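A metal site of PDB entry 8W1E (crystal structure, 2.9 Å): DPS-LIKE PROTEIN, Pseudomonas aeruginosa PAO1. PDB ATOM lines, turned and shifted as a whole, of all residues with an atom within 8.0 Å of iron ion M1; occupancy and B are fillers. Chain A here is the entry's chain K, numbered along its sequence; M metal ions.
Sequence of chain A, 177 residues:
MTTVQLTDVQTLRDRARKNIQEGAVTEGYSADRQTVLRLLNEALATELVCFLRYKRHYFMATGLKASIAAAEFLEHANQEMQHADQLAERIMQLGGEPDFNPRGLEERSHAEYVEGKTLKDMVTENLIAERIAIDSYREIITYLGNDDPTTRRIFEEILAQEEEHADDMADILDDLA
The side-chain hydroxyl (OH) of Tyr 137 lies within hydrogen-bond range of the side-chain carboxylate (OE1) of Glu 47.
The side-chain sulfur of Cys 50 lies close to the side-chain carboxylate of Glu 80, at 3.7 Å.
Glu 162 touches iron ion M1.
Along chain A the residues within 4 Å of iron ion M1 span positions 47 to 162.
The nearest printed residue that does not touch iron ion M1 is Ile 158 (4.3 Å).
Iron ion M1 is bound by the side-chain carboxylate (OE2) of Glu 47, a ring nitrogen (ND1) of His 83 and the side-chain carboxylate (OE1) of Glu 80.
Iron ion M1 has three donor atoms within binding distance.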
ATOM      1  N   ALA A  43      23.427  23.532 -10.787  1.00  0.00           N
ATOM      2  CA  ALA A  43      24.076  23.108 -12.024  1.00  0.00           C
ATOM      3  C   ALA A  43      23.308  23.633 -13.230  1.00  0.00           C
ATOM      4  O   ALA A  43      23.923  24.124 -14.197  1.00  0.00           O
ATOM      5  CB  ALA A  43      24.174  21.584 -12.075  1.00  0.00           C
ATOM      6  N   THR A  46      24.185  27.185 -13.770  1.00  0.00           N
ATOM      7  CA  THR A  46      25.540  27.296 -14.312  1.00  0.00           C
ATOM      8  C   THR A  46      25.575  27.031 -15.817  1.00  0.00           C
ATOM      9  O   THR A  46      26.278  27.728 -16.563  1.00  0.00           O
ATOM     10  CB  THR A  46      26.481  26.329 -13.582  1.00  0.00           C
ATOM     11  OG1 THR A  46      26.560  26.710 -12.204  1.00  0.00           O
ATOM     12  CG2 THR A  46      27.865  26.373 -14.220  1.00  0.00           C
ATOM     13  N   GLU A  47      24.854  26.010 -16.280  1.00  0.00           N
ATOM     14  CA  GLU A  47      24.908  25.687 -17.705  1.00  0.00           C
ATOM     15  C   GLU A  47      24.208  26.753 -18.530  1.00  0.00           C
ATOM     16  O   GLU A  47      24.667  27.101 -19.622  1.00  0.00           O
ATOM     17  CB  GLU A  47      24.288  24.321 -17.968  1.00  0.00           C
ATOM     18  CG  GLU A  47      24.848  23.256 -17.060  1.00  0.00           C
ATOM     19  CD  GLU A  47      26.330  23.019 -17.219  1.00  0.00           C
ATOM     20  OE1 GLU A  47      27.140  23.958 -17.047  1.00  0.00           O
ATOM     21  OE2 GLU A  47      26.687  21.862 -17.471  1.00  0.00           O
ATOM     22  N   LEU A  48      23.075  27.273 -18.049  1.00  0.00           N
ATOM     23  CA  LEU A  48      22.372  28.327 -18.796  1.00  0.00           C
ATOM     24  C   LEU A  48      23.247  29.572 -18.938  1.00  0.00           C
ATOM     25  O   LEU A  48      23.335  30.154 -20.025  1.00  0.00           O
ATOM     26  CB  LEU A  48      21.058  28.677 -18.113  1.00  0.00           C
ATOM     27  CG  LEU A  48      20.026  27.547 -18.152  1.00  0.00           C
ATOM     28  CD1 LEU A  48      18.763  27.886 -17.384  1.00  0.00           C
ATOM     29  CD2 LEU A  48      19.701  27.177 -19.597  1.00  0.00           C
ATOM     30  N   CYS A  50      26.647  29.632 -18.713  1.00  0.00           N
ATOM     31  CA  CYS A  50      27.742  29.273 -19.617  1.00  0.00           C
ATOM     32  C   CYS A  50      27.284  29.269 -21.073  1.00  0.00           C
ATOM     33  O   CYS A  50      28.027  29.677 -21.973  1.00  0.00           O
ATOM     34  CB  CYS A  50      28.334  27.911 -19.237  1.00  0.00           C
ATOM     35  SG  CYS A  50      29.499  27.868 -17.814  1.00  0.00           S
ATOM     36  N   PHE A  51      26.040  28.832 -21.342  1.00  0.00           N
ATOM     37  CA  PHE A  51      25.491  28.895 -22.693  1.00  0.00           C
ATOM     38  C   PHE A  51      25.414  30.332 -23.189  1.00  0.00           C
ATOM     39  O   PHE A  51      25.812  30.638 -24.321  1.00  0.00           O
ATOM     40  CB  PHE A  51      24.100  28.259 -22.727  1.00  0.00           C
ATOM     41  CG  PHE A  51      23.352  28.519 -23.996  1.00  0.00           C
ATOM     42  CD1 PHE A  51      23.482  27.679 -25.082  1.00  0.00           C
ATOM     43  CD2 PHE A  51      22.528  29.629 -24.108  1.00  0.00           C
ATOM     44  CE1 PHE A  51      22.810  27.923 -26.253  1.00  0.00           C
ATOM     45  CE2 PHE A  51      21.843  29.875 -25.286  1.00  0.00           C
ATOM     46  CZ  PHE A  51      21.988  29.028 -26.357  1.00  0.00           C
ATOM     47  N   TYR A  54      29.014  31.783 -23.866  1.00  0.00           N
ATOM     48  CA  TYR A  54      29.613  31.236 -25.084  1.00  0.00           C
ATOM     49  C   TYR A  54      28.917  31.772 -26.332  1.00  0.00           C
ATOM     50  O   TYR A  54      29.569  32.036 -27.344  1.00  0.00           O
ATOM     51  CB  TYR A  54      29.537  29.708 -25.068  1.00  0.00           C
ATOM     52  CG  TYR A  54      30.702  28.997 -24.422  1.00  0.00           C
ATOM     53  CD1 TYR A  54      31.988  29.150 -24.893  1.00  0.00           C
ATOM     54  CD2 TYR A  54      30.493  28.119 -23.357  1.00  0.00           C
ATOM     55  CE1 TYR A  54      33.038  28.484 -24.304  1.00  0.00           C
ATOM     56  CE2 TYR A  54      31.532  27.446 -22.779  1.00  0.00           C
ATOM     57  CZ  TYR A  54      32.809  27.634 -23.251  1.00  0.00           C
ATOM     58  OH  TYR A  54      33.857  26.964 -22.675  1.00  0.00           O
ATOM     59  N   HIS A  76      30.784  24.371 -27.750  1.00  0.00           N
ATOM     60  CA  HIS A  76      30.653  24.339 -26.299  1.00  0.00           C
ATOM     61  C   HIS A  76      29.265  24.822 -25.886  1.00  0.00           C
ATOM     62  O   HIS A  76      28.572  24.160 -25.100  1.00  0.00           O
ATOM     63  CB  HIS A  76      31.756  25.180 -25.657  1.00  0.00           C
ATOM     64  CG  HIS A  76      33.117  24.571 -25.773  1.00  0.00           C
ATOM     65  ND1 HIS A  76      34.174  24.945 -24.975  1.00  0.00           N
ATOM     66  CD2 HIS A  76      33.598  23.640 -26.620  1.00  0.00           C
ATOM     67  CE1 HIS A  76      35.249  24.260 -25.315  1.00  0.00           C
ATOM     68  NE2 HIS A  76      34.926  23.453 -26.316  1.00  0.00           N
ATOM     69  N   ALA A  77      28.823  25.956 -26.423  1.00  0.00           N
ATOM     70  CA  ALA A  77      27.521  26.493 -26.043  1.00  0.00           C
ATOM     71  C   ALA A  77      26.432  25.438 -26.177  1.00  0.00           C
ATOM     72  O   ALA A  77      25.619  25.239 -25.266  1.00  0.00           O
ATOM     73  CB  ALA A  77      27.176  27.707 -26.902  1.00  0.00           C
ATOM     74  N   ASN A  78      26.389  24.756 -27.307  1.00  0.00           N
ATOM     75  CA  ASN A  78      25.295  23.818 -27.480  1.00  0.00           C
ATOM     76  C   ASN A  78      25.460  22.610 -26.571  1.00  0.00           C
ATOM     77  O   ASN A  78      24.472  22.063 -26.088  1.00  0.00           O
ATOM     78  CB  ASN A  78      25.165  23.436 -28.961  1.00  0.00           C
ATOM     79  CG  ASN A  78      24.717  24.620 -29.850  1.00  0.00           C
ATOM     80  OD1 ASN A  78      23.916  25.483 -29.439  1.00  0.00           O
ATOM     81  ND2 ASN A  78      25.216  24.645 -31.080  1.00  0.00           N
ATOM     82  N   GLN A  79      26.704  22.200 -26.283  1.00  0.00           N
ATOM     83  CA  GLN A  79      26.880  21.143 -25.291  1.00  0.00           C
ATOM     84  C   GLN A  79      26.386  21.590 -23.925  1.00  0.00           C
ATOM     85  O   GLN A  79      25.842  20.778 -23.154  1.00  0.00           O
ATOM     86  CB  GLN A  79      28.352  20.702 -25.216  1.00  0.00           C
ATOM     87  CG  GLN A  79      28.694  19.448 -26.045  1.00  0.00           C
ATOM     88  CD  GLN A  79      30.018  19.609 -26.848  1.00  0.00           C
ATOM     89  OE1 GLN A  79      30.963  20.270 -26.388  1.00  0.00           O
ATOM     90  NE2 GLN A  79      30.065  19.019 -28.051  1.00  0.00           N
ATOM     91  N   GLU A  80      26.593  22.873 -23.573  1.00  0.00           N
ATOM     92  CA  GLU A  80      26.087  23.386 -22.297  1.00  0.00           C
ATOM     93  C   GLU A  80      24.567  23.236 -22.226  1.00  0.00           C
ATOM     94  O   GLU A  80      24.028  22.829 -21.190  1.00  0.00           O
ATOM     95  CB  GLU A  80      26.444  24.858 -22.126  1.00  0.00           C
ATOM     96  CG  GLU A  80      27.908  25.218 -22.167  1.00  0.00           C
ATOM     97  CD  GLU A  80      28.725  24.461 -21.168  1.00  0.00           C
ATOM     98  OE1 GLU A  80      28.810  23.235 -21.345  1.00  0.00           O
ATOM     99  OE2 GLU A  80      29.271  25.079 -20.218  1.00  0.00           O
ATOM    100  N   MET A  81      23.872  23.546 -23.317  1.00  0.00           N
ATOM    101  CA  MET A  81      22.429  23.444 -23.328  1.00  0.00           C
ATOM    102  C   MET A  81      21.975  21.997 -23.213  1.00  0.00           C
ATOM    103  O   MET A  81      20.962  21.711 -22.585  1.00  0.00           O
ATOM    104  CB  MET A  81      21.863  24.093 -24.579  1.00  0.00           C
ATOM    105  CG  MET A  81      20.385  24.392 -24.482  1.00  0.00           C
ATOM    106  SD  MET A  81      20.064  25.806 -23.448  1.00  0.00           S
ATOM    107  CE  MET A  81      18.627  25.209 -22.534  1.00  0.00           C
ATOM    108  N   GLN A  82      22.718  21.063 -23.848  1.00  0.00           N
ATOM    109  CA  GLN A  82      22.419  19.652 -23.645  1.00  0.00           C
ATOM    110  C   GLN A  82      22.533  19.272 -22.173  1.00  0.00           C
ATOM    111  O   GLN A  82      21.710  18.501 -21.658  1.00  0.00           O
ATOM    112  CB  GLN A  82      23.344  18.763 -24.471  1.00  0.00           C
ATOM    113  CG  GLN A  82      22.837  18.498 -25.856  1.00  0.00           C
ATOM    114  CD  GLN A  82      23.873  17.830 -26.749  1.00  0.00           C
ATOM    115  OE1 GLN A  82      24.784  18.476 -27.293  1.00  0.00           O
ATOM    116  NE2 GLN A  82      23.736  16.510 -26.893  1.00  0.00           N
ATOM    117  N   HIS A  83      23.557  19.783 -21.490  1.00  0.00           N
ATOM    118  CA  HIS A  83      23.681  19.548 -20.060  1.00  0.00           C
ATOM    119  C   HIS A  83      22.495  20.143 -19.327  1.00  0.00           C
ATOM    120  O   HIS A  83      21.898  19.499 -18.454  1.00  0.00           O
ATOM    121  CB  HIS A  83      24.988  20.129 -19.550  1.00  0.00           C
ATOM    122  CG  HIS A  83      26.207  19.523 -20.181  1.00  0.00           C
ATOM    123  ND1 HIS A  83      27.451  20.087 -20.080  1.00  0.00           N
ATOM    124  CD2 HIS A  83      26.355  18.406 -20.927  1.00  0.00           C
ATOM    125  CE1 HIS A  83      28.322  19.345 -20.732  1.00  0.00           C
ATOM    126  NE2 HIS A  83      27.683  18.317 -21.263  1.00  0.00           N
ATOM    127  N   ALA A  84      22.096  21.367 -19.694  1.00  0.00           N
ATOM    128  CA  ALA A  84      20.931  21.992 -19.083  1.00  0.00           C
ATOM    129  C   ALA A  84      19.715  21.094 -19.192  1.00  0.00           C
ATOM    130  O   ALA A  84      18.960  20.917 -18.228  1.00  0.00           O
ATOM    131  CB  ALA A  84      20.663  23.339 -19.759  1.00  0.00           C
ATOM    132  N   LEU A  87      19.947  17.974 -16.917  1.00  0.00           N
ATOM    133  CA  LEU A  87      19.735  18.320 -15.523  1.00  0.00           C
ATOM    134  C   LEU A  87      18.268  18.624 -15.258  1.00  0.00           C
ATOM    135  O   LEU A  87      17.705  18.156 -14.260  1.00  0.00           O
ATOM    136  CB  LEU A  87      20.626  19.508 -15.164  1.00  0.00           C
ATOM    137  CG  LEU A  87      22.137  19.260 -15.243  1.00  0.00           C
ATOM    138  CD1 LEU A  87      22.898  20.565 -15.409  1.00  0.00           C
ATOM    139  CD2 LEU A  87      22.669  18.523 -14.007  1.00  0.00           C
ATOM    140  N   GLU A 130      34.956  26.766 -16.909  1.00  0.00           N
ATOM    141  CA  GLU A 130      35.055  25.316 -16.967  1.00  0.00           C
ATOM    142  C   GLU A 130      35.750  24.768 -15.737  1.00  0.00           C
ATOM    143  O   GLU A 130      35.353  23.734 -15.189  1.00  0.00           O
ATOM    144  CB  GLU A 130      35.788  24.872 -18.230  1.00  0.00           C
ATOM    145  CG  GLU A 130      35.247  25.396 -19.562  1.00  0.00           C
ATOM    146  CD  GLU A 130      33.832  24.945 -19.865  1.00  0.00           C
ATOM    147  OE1 GLU A 130      33.237  24.227 -19.023  1.00  0.00           O
ATOM    148  OE2 GLU A 130      33.323  25.261 -20.965  1.00  0.00           O
ATOM    149  N   ALA A 133      33.376  24.799 -12.919  1.00  0.00           N
ATOM    150  CA  ALA A 133      32.418  23.710 -13.067  1.00  0.00           C
ATOM    151  C   ALA A 133      33.057  22.361 -12.755  1.00  0.00           C
ATOM    152  O   ALA A 133      32.459  21.540 -12.055  1.00  0.00           O
ATOM    153  CB  ALA A 133      31.862  23.701 -14.494  1.00  0.00           C
ATOM    154  N   TYR A 137      31.431  20.063  -9.909  1.00  0.00           N
ATOM    155  CA  TYR A 137      30.764  18.793 -10.186  1.00  0.00           C
ATOM    156  C   TYR A 137      31.524  17.609  -9.580  1.00  0.00           C
ATOM    157  O   TYR A 137      30.885  16.616  -9.204  1.00  0.00           O
ATOM    158  CB  TYR A 137      30.605  18.637 -11.696  1.00  0.00           C
ATOM    159  CG  TYR A 137      29.749  19.719 -12.328  1.00  0.00           C
ATOM    160  CD1 TYR A 137      28.839  20.443 -11.577  1.00  0.00           C
ATOM    161  CD2 TYR A 137      29.859  20.012 -13.671  1.00  0.00           C
ATOM    162  CE1 TYR A 137      28.052  21.425 -12.146  1.00  0.00           C
ATOM    163  CE2 TYR A 137      29.078  21.001 -14.250  1.00  0.00           C
ATOM    164  CZ  TYR A 137      28.175  21.707 -13.487  1.00  0.00           C
ATOM    165  OH  TYR A 137      27.397  22.690 -14.058  1.00  0.00           O
ATOM    166  N   ILE A 158      28.774  14.918 -17.550  1.00  0.00           N
ATOM    167  CA  ILE A 158      28.993  16.357 -17.699  1.00  0.00           C
ATOM    168  C   ILE A 158      30.424  16.717 -17.321  1.00  0.00           C
ATOM    169  O   ILE A 158      31.110  17.462 -18.034  1.00  0.00           O
ATOM    170  CB  ILE A 158      27.961  17.134 -16.866  1.00  0.00           C
ATOM    171  CG1 ILE A 158      26.555  16.921 -17.420  1.00  0.00           C
ATOM    172  CG2 ILE A 158      28.308  18.613 -16.843  1.00  0.00           C
ATOM    173  CD1 ILE A 158      25.455  17.482 -16.556  1.00  0.00           C
ATOM    174  N   LEU A 159      30.897  16.187 -16.187  1.00  0.00           N
ATOM    175  CA  LEU A 159      32.262  16.463 -15.763  1.00  0.00           C
ATOM    176  C   LEU A 159      33.232  16.188 -16.889  1.00  0.00           C
ATOM    177  O   LEU A 159      34.101  17.011 -17.210  1.00  0.00           O
ATOM    178  CB  LEU A 159      32.604  15.580 -14.559  1.00  0.00           C
ATOM    179  CG  LEU A 159      34.083  15.522 -14.184  1.00  0.00           C
ATOM    180  CD1 LEU A 159      34.579  16.899 -13.790  1.00  0.00           C
ATOM    181  CD2 LEU A 159      34.301  14.522 -13.065  1.00  0.00           C
ATOM    182  N   GLN A 161      32.801  16.118 -20.021  1.00  0.00           N
ATOM    183  CA  GLN A 161      32.702  17.115 -21.073  1.00  0.00           C
ATOM    184  C   GLN A 161      33.375  18.428 -20.654  1.00  0.00           C
ATOM    185  O   GLN A 161      34.034  19.071 -21.476  1.00  0.00           O
ATOM    186  CB  GLN A 161      31.238  17.340 -21.430  1.00  0.00           C
ATOM    187  CG  GLN A 161      31.031  18.275 -22.576  1.00  0.00           C
ATOM    188  CD  GLN A 161      31.244  17.612 -23.876  1.00  0.00           C
ATOM    189  OE1 GLN A 161      30.340  16.956 -24.394  1.00  0.00           O
ATOM    190  NE2 GLN A 161      32.445  17.719 -24.405  1.00  0.00           N
ATOM    191  N   GLU A 162      33.193  18.840 -19.400  1.00  0.00           N
ATOM    192  CA  GLU A 162      33.792  20.092 -18.955  1.00  0.00           C
ATOM    193  C   GLU A 162      35.308  19.997 -18.973  1.00  0.00           C
ATOM    194  O   GLU A 162      35.992  20.977 -19.299  1.00  0.00           O
ATOM    195  CB  GLU A 162      33.335  20.461 -17.551  1.00  0.00           C
ATOM    196  CG  GLU A 162      31.821  20.554 -17.355  1.00  0.00           C
ATOM    197  CD  GLU A 162      31.171  21.582 -18.242  1.00  0.00           C
ATOM    198  OE1 GLU A 162      31.165  21.364 -19.467  1.00  0.00           O
ATOM    199  OE2 GLU A 162      30.702  22.626 -17.731  1.00  0.00           O
ATOM    200  N   HIS A 165      36.186  20.735 -22.390  1.00  0.00           N
ATOM    201  CA  HIS A 165      36.051  22.157 -22.660  1.00  0.00           C
ATOM    202  C   HIS A 165      37.223  22.939 -22.062  1.00  0.00           C
ATOM    203  O   HIS A 165      37.735  23.876 -22.680  1.00  0.00           O
ATOM    204  CB  HIS A 165      34.711  22.667 -22.128  1.00  0.00           C
ATOM    205  CG  HIS A 165      33.526  22.185 -22.909  1.00  0.00           C
ATOM    206  ND1 HIS A 165      32.230  22.438 -22.526  1.00  0.00           N
ATOM    207  CD2 HIS A 165      33.442  21.487 -24.059  1.00  0.00           C
ATOM    208  CE1 HIS A 165      31.393  21.913 -23.399  1.00  0.00           C
ATOM    209  NE2 HIS A 165      32.106  21.329 -24.341  1.00  0.00           N
HETATM  210 FE    FE M   1      28.258  22.215 -19.192  1.00  0.00          FE
HETATM  211 FE    FE M   2      31.547  23.515 -20.535  1.00  0.00          FE
